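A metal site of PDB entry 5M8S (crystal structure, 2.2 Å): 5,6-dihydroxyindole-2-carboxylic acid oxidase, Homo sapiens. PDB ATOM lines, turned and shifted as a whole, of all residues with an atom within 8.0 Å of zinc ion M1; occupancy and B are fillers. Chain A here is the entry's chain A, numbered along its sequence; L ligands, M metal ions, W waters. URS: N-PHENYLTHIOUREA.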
ATOM      1  N   HIS A 168      14.238 -21.961   7.341  1.00  0.00           N
ATOM      2  CA  HIS A 168      13.318 -21.046   8.010  1.00  0.00           C
ATOM      3  C   HIS A 168      11.883 -21.498   7.787  1.00  0.00           C
ATOM      4  O   HIS A 168      11.084 -21.572   8.735  1.00  0.00           O
ATOM      5  CB  HIS A 168      13.524 -19.627   7.474  1.00  0.00           C
ATOM      6  CG  HIS A 168      12.936 -18.523   8.316  1.00  0.00           C
ATOM      7  ND1 HIS A 168      11.655 -18.023   8.113  1.00  0.00           N
ATOM      8  CD2 HIS A 168      13.468 -17.795   9.323  1.00  0.00           C
ATOM      9  CE1 HIS A 168      11.444 -17.034   8.968  1.00  0.00           C
ATOM     10  NE2 HIS A 168      12.527 -16.871   9.709  1.00  0.00           N
ATOM     11  N   SER A 190      11.011 -21.086  15.711  1.00  0.00           N
ATOM     12  CA  SER A 190      12.014 -20.016  15.621  1.00  0.00           C
ATOM     13  C   SER A 190      11.475 -18.631  15.926  1.00  0.00           C
ATOM     14  O   SER A 190      12.248 -17.656  15.861  1.00  0.00           O
ATOM     15  CB  SER A 190      12.638 -20.010  14.213  1.00  0.00           C
ATOM     16  OG  SER A 190      11.624 -19.950  13.229  1.00  0.00           O
ATOM     17  N   HIS A 191      10.186 -18.487  16.249  1.00  0.00           N
ATOM     18  CA  HIS A 191       9.591 -17.198  16.570  1.00  0.00           C
ATOM     19  C   HIS A 191       8.656 -17.365  17.745  1.00  0.00           C
ATOM     20  O   HIS A 191       8.310 -18.488  18.134  1.00  0.00           O
ATOM     21  CB  HIS A 191       8.808 -16.614  15.395  1.00  0.00           C
ATOM     22  CG  HIS A 191       9.586 -16.580  14.130  1.00  0.00           C
ATOM     23  ND1 HIS A 191       9.755 -17.687  13.322  1.00  0.00           N
ATOM     24  CD2 HIS A 191      10.327 -15.591  13.563  1.00  0.00           C
ATOM     25  CE1 HIS A 191      10.507 -17.366  12.283  1.00  0.00           C
ATOM     26  NE2 HIS A 191      10.858 -16.100  12.407  1.00  0.00           N
ATOM     27  N   PHE A 196      13.960 -17.191  19.482  1.00  0.00           N
ATOM     28  CA  PHE A 196      13.923 -16.323  18.297  1.00  0.00           C
ATOM     29  C   PHE A 196      15.316 -15.771  17.981  1.00  0.00           C
ATOM     30  O   PHE A 196      15.764 -15.838  16.830  1.00  0.00           O
ATOM     31  CB  PHE A 196      12.916 -15.187  18.515  1.00  0.00           C
ATOM     32  CG  PHE A 196      13.053 -14.052  17.542  1.00  0.00           C
ATOM     33  CD1 PHE A 196      12.635 -14.201  16.230  1.00  0.00           C
ATOM     34  CD2 PHE A 196      13.602 -12.833  17.934  1.00  0.00           C
ATOM     35  CE1 PHE A 196      12.749 -13.143  15.307  1.00  0.00           C
ATOM     36  CE2 PHE A 196      13.727 -11.773  17.021  1.00  0.00           C
ATOM     37  CZ  PHE A 196      13.292 -11.934  15.706  1.00  0.00           C
ATOM     38  N   HIS A 200      17.905 -17.309  14.826  1.00  0.00           N
ATOM     39  CA  HIS A 200      18.283 -16.473  13.683  1.00  0.00           C
ATOM     40  C   HIS A 200      19.766 -16.167  13.683  1.00  0.00           C
ATOM     41  O   HIS A 200      20.359 -15.982  12.622  1.00  0.00           O
ATOM     42  CB  HIS A 200      17.445 -15.203  13.672  1.00  0.00           C
ATOM     43  CG  HIS A 200      16.019 -15.445  13.305  1.00  0.00           C
ATOM     44  ND1 HIS A 200      15.105 -15.954  14.198  1.00  0.00           N
ATOM     45  CD2 HIS A 200      15.355 -15.270  12.142  1.00  0.00           C
ATOM     46  CE1 HIS A 200      13.932 -16.094  13.602  1.00  0.00           C
ATOM     47  NE2 HIS A 200      14.056 -15.683  12.352  1.00  0.00           N
ATOM     48  N   HIS A 203      21.182 -19.204  11.995  1.00  0.00           N
ATOM     49  CA  HIS A 203      20.735 -19.048  10.612  1.00  0.00           C
ATOM     50  C   HIS A 203      21.707 -18.151   9.824  1.00  0.00           C
ATOM     51  O   HIS A 203      22.183 -18.540   8.746  1.00  0.00           O
ATOM     52  CB  HIS A 203      19.315 -18.483  10.629  1.00  0.00           C
ATOM     53  CG  HIS A 203      18.557 -18.607   9.332  1.00  0.00           C
ATOM     54  ND1 HIS A 203      17.685 -17.639   8.890  1.00  0.00           N
ATOM     55  CD2 HIS A 203      18.486 -19.611   8.426  1.00  0.00           C
ATOM     56  CE1 HIS A 203      17.134 -18.017   7.754  1.00  0.00           C
ATOM     57  NE2 HIS A 203      17.607 -19.207   7.441  1.00  0.00           N
ATOM     58  N   GLU A 336      11.826  -8.577  19.180  1.00  0.00           N
ATOM     59  CA  GLU A 336      11.081  -9.299  18.150  1.00  0.00           C
ATOM     60  C   GLU A 336       9.937  -8.438  17.614  1.00  0.00           C
ATOM     61  O   GLU A 336       9.644  -8.448  16.412  1.00  0.00           O
ATOM     62  CB  GLU A 336      10.544 -10.636  18.691  1.00  0.00           C
ATOM     63  CG  GLU A 336       9.829 -11.480  17.599  1.00  0.00           C
ATOM     64  CD  GLU A 336       9.539 -12.941  18.013  1.00  0.00           C
ATOM     65  OE1 GLU A 336       9.757 -13.288  19.196  1.00  0.00           O
ATOM     66  OE2 GLU A 336       9.082 -13.739  17.159  1.00  0.00           O
ATOM     67  N   HIS A 353      11.682  -5.507  14.923  1.00  0.00           N
ATOM     68  CA  HIS A 353      11.832  -6.566  13.927  1.00  0.00           C
ATOM     69  C   HIS A 353      10.528  -6.872  13.209  1.00  0.00           C
ATOM     70  O   HIS A 353      10.485  -6.950  11.972  1.00  0.00           O
ATOM     71  CB  HIS A 353      12.395  -7.818  14.597  1.00  0.00           C
ATOM     72  CG  HIS A 353      12.091  -9.101  13.870  1.00  0.00           C
ATOM     73  ND1 HIS A 353      10.976  -9.861  14.138  1.00  0.00           N
ATOM     74  CD2 HIS A 353      12.806  -9.788  12.949  1.00  0.00           C
ATOM     75  CE1 HIS A 353      10.985 -10.941  13.381  1.00  0.00           C
ATOM     76  NE2 HIS A 353      12.083 -10.912  12.642  1.00  0.00           N
ATOM     77  N   ASN A 354       9.437  -7.050  13.969  1.00  0.00           N
ATOM     78  CA  ASN A 354       8.167  -7.359  13.320  1.00  0.00           C
ATOM     79  C   ASN A 354       7.732  -6.207  12.405  1.00  0.00           C
ATOM     80  O   ASN A 354       7.251  -6.446  11.292  1.00  0.00           O
ATOM     81  CB  ASN A 354       7.087  -7.686  14.347  1.00  0.00           C
ATOM     82  CG  ASN A 354       7.205  -9.114  14.912  1.00  0.00           C
ATOM     83  OD1 ASN A 354       7.966  -9.946  14.408  1.00  0.00           O
ATOM     84  ND2 ASN A 354       6.430  -9.419  15.941  1.00  0.00           N
ATOM     85  N   ALA A 356       9.700  -3.938  10.889  1.00  0.00           N
ATOM     86  CA  ALA A 356      10.540  -3.877   9.700  1.00  0.00           C
ATOM     87  C   ALA A 356      10.077  -4.886   8.663  1.00  0.00           C
ATOM     88  O   ALA A 356      10.028  -4.584   7.463  1.00  0.00           O
ATOM     89  CB  ALA A 356      12.012  -4.093  10.064  1.00  0.00           C
ATOM     90  N   HIS A 357       9.681  -6.084   9.109  1.00  0.00           N
ATOM     91  CA  HIS A 357       9.131  -7.074   8.203  1.00  0.00           C
ATOM     92  C   HIS A 357       7.858  -6.569   7.539  1.00  0.00           C
ATOM     93  O   HIS A 357       7.722  -6.621   6.302  1.00  0.00           O
ATOM     94  CB  HIS A 357       8.839  -8.380   8.945  1.00  0.00           C
ATOM     95  CG  HIS A 357       9.981  -9.354   8.992  1.00  0.00           C
ATOM     96  ND1 HIS A 357      10.412 -10.039   7.882  1.00  0.00           N
ATOM     97  CD2 HIS A 357      10.698  -9.831  10.029  1.00  0.00           C
ATOM     98  CE1 HIS A 357      11.379 -10.872   8.227  1.00  0.00           C
ATOM     99  NE2 HIS A 357      11.576 -10.756   9.523  1.00  0.00           N
ATOM    100  N   GLY A 364       8.886 -10.349   1.736  1.00  0.00           N
ATOM    101  CA  GLY A 364       9.694 -10.233   2.950  1.00  0.00           C
ATOM    102  C   GLY A 364       8.896 -10.017   4.219  1.00  0.00           C
ATOM    103  O   GLY A 364       9.480 -10.022   5.310  1.00  0.00           O
ATOM    104  N   SER A 370       9.440 -14.996   4.061  1.00  0.00           N
ATOM    105  CA  SER A 370      10.233 -13.782   4.222  1.00  0.00           C
ATOM    106  C   SER A 370      11.696 -13.900   3.801  1.00  0.00           C
ATOM    107  O   SER A 370      12.181 -12.957   3.151  1.00  0.00           O
ATOM    108  CB  SER A 370      10.084 -13.269   5.657  1.00  0.00           C
ATOM    109  OG  SER A 370      10.434 -14.242   6.651  1.00  0.00           O
ATOM    110  N   PRO A 371      12.432 -15.002   4.046  1.00  0.00           N
ATOM    111  CA  PRO A 371      13.837 -15.036   3.598  1.00  0.00           C
ATOM    112  C   PRO A 371      13.999 -15.009   2.088  1.00  0.00           C
ATOM    113  O   PRO A 371      15.123 -14.786   1.610  1.00  0.00           O
ATOM    114  CB  PRO A 371      14.370 -16.353   4.157  1.00  0.00           C
ATOM    115  CG  PRO A 371      13.399 -16.766   5.208  1.00  0.00           C
ATOM    116  CD  PRO A 371      12.079 -16.252   4.739  1.00  0.00           C
ATOM    117  N   PHE A 376      15.834  -9.728   4.070  1.00  0.00           N
ATOM    118  CA  PHE A 376      15.790 -10.539   5.288  1.00  0.00           C
ATOM    119  C   PHE A 376      17.181 -10.672   5.911  1.00  0.00           C
ATOM    120  O   PHE A 376      17.320 -10.552   7.133  1.00  0.00           O
ATOM    121  CB  PHE A 376      15.213 -11.933   4.960  1.00  0.00           C
ATOM    122  CG  PHE A 376      15.147 -12.880   6.145  1.00  0.00           C
ATOM    123  CD1 PHE A 376      16.268 -13.576   6.570  1.00  0.00           C
ATOM    124  CD2 PHE A 376      13.935 -13.134   6.766  1.00  0.00           C
ATOM    125  CE1 PHE A 376      16.209 -14.451   7.629  1.00  0.00           C
ATOM    126  CE2 PHE A 376      13.857 -14.034   7.818  1.00  0.00           C
ATOM    127  CZ  PHE A 376      15.002 -14.679   8.259  1.00  0.00           C
ATOM    128  N   LEU A 379      18.116  -7.342   7.516  1.00  0.00           N
ATOM    129  CA  LEU A 379      17.208  -7.111   8.629  1.00  0.00           C
ATOM    130  C   LEU A 379      17.630  -7.917   9.848  1.00  0.00           C
ATOM    131  O   LEU A 379      17.584  -7.428  10.978  1.00  0.00           O
ATOM    132  CB  LEU A 379      15.786  -7.470   8.186  1.00  0.00           C
ATOM    133  CG  LEU A 379      14.564  -7.153   9.053  1.00  0.00           C
ATOM    134  CD1 LEU A 379      13.312  -7.189   8.197  1.00  0.00           C
ATOM    135  CD2 LEU A 379      14.409  -8.165  10.231  1.00  0.00           C
ATOM    136  N   HIS A 380      18.099  -9.148   9.641  1.00  0.00           N
ATOM    137  CA  HIS A 380      18.411  -9.983  10.795  1.00  0.00           C
ATOM    138  C   HIS A 380      19.854  -9.863  11.283  1.00  0.00           C
ATOM    139  O   HIS A 380      20.102 -10.166  12.457  1.00  0.00           O
ATOM    140  CB  HIS A 380      18.070 -11.455  10.543  1.00  0.00           C
ATOM    141  CG  HIS A 380      16.660 -11.783  10.908  1.00  0.00           C
ATOM    142  ND1 HIS A 380      16.255 -11.930  12.222  1.00  0.00           N
ATOM    143  CD2 HIS A 380      15.550 -11.889  10.154  1.00  0.00           C
ATOM    144  CE1 HIS A 380      14.954 -12.166  12.242  1.00  0.00           C
ATOM    145  NE2 HIS A 380      14.508 -12.148  11.011  1.00  0.00           N
ATOM    146  N   THR A 383      19.138  -7.054  13.686  1.00  0.00           N
ATOM    147  CA  THR A 383      18.485  -7.647  14.849  1.00  0.00           C
ATOM    148  C   THR A 383      19.501  -8.398  15.701  1.00  0.00           C
ATOM    149  O   THR A 383      19.450  -8.360  16.932  1.00  0.00           O
ATOM    150  CB  THR A 383      17.382  -8.587  14.393  1.00  0.00           C
ATOM    151  OG1 THR A 383      16.467  -7.890  13.548  1.00  0.00           O
ATOM    152  CG2 THR A 383      16.612  -9.159  15.604  1.00  0.00           C
HETATM  153  N1  URS L   1       6.530 -11.501  10.656  1.00  0.00           N
HETATM  154  N2  URS L   1       5.054 -10.953   8.881  1.00  0.00           N
HETATM  155  C1  URS L   1       3.977 -11.692  13.463  1.00  0.00           C
HETATM  156  C2  URS L   1       4.998 -12.069  12.404  1.00  0.00           C
HETATM  157  C3  URS L   1       5.551 -11.143  11.663  1.00  0.00           C
HETATM  158  C4  URS L   1       5.159  -9.690  11.839  1.00  0.00           C
HETATM  159  C5  URS L   1       4.274  -9.347  12.737  1.00  0.00           C
HETATM  160  C6  URS L   1       3.648 -10.425  13.607  1.00  0.00           C
HETATM  161  C7  URS L   1       6.199 -11.366   9.247  1.00  0.00           C
HETATM  162  S1  URS L   1       7.309 -11.762   8.169  1.00  0.00           S
HETATM  163 ZN    ZN M   1      12.519 -11.942  10.882  1.00  0.00          ZN
HETATM  164 ZN    ZN M   2      12.378 -15.483  11.145  1.00  0.00          ZN
HETATM  165  O   HOH W   1      11.637 -13.742  10.468  1.00  0.00           O
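Zinc ion M1 is bound by a ring nitrogen (NE2) of His 380, a ring nitrogen (NE2) of His 357, water W1 and a ring nitrogen (NE2) of His 353. Zinc ion M1 has four donor atoms within binding distance.
The side-chain amide oxygen (OD1) of Asn 354 sits at hydrogen-bond distance from a ring nitrogen (ND1) of His 353 (3.0 Å). ND1 of His 353 is in hydrogen-bond range of O of Glu 336, at 3.0 Å. A ring nitrogen (ND1) of His 357 is in hydrogen-bond range of the backbone carbonyl oxygen (O) of Gly 364 (2.7 Å).
ND1 of His 357 lies close to S1 of the ligand, 3.6 Å away.
CE2 of Phe 376 touches zinc ion M1 (3.9 Å). Within 4 Å of zinc ion M1: His 353, His 357, Phe 376 and His 380. The nearest printed residue that does not touch zinc ion M1 is Leu 379 (4.3 Å).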
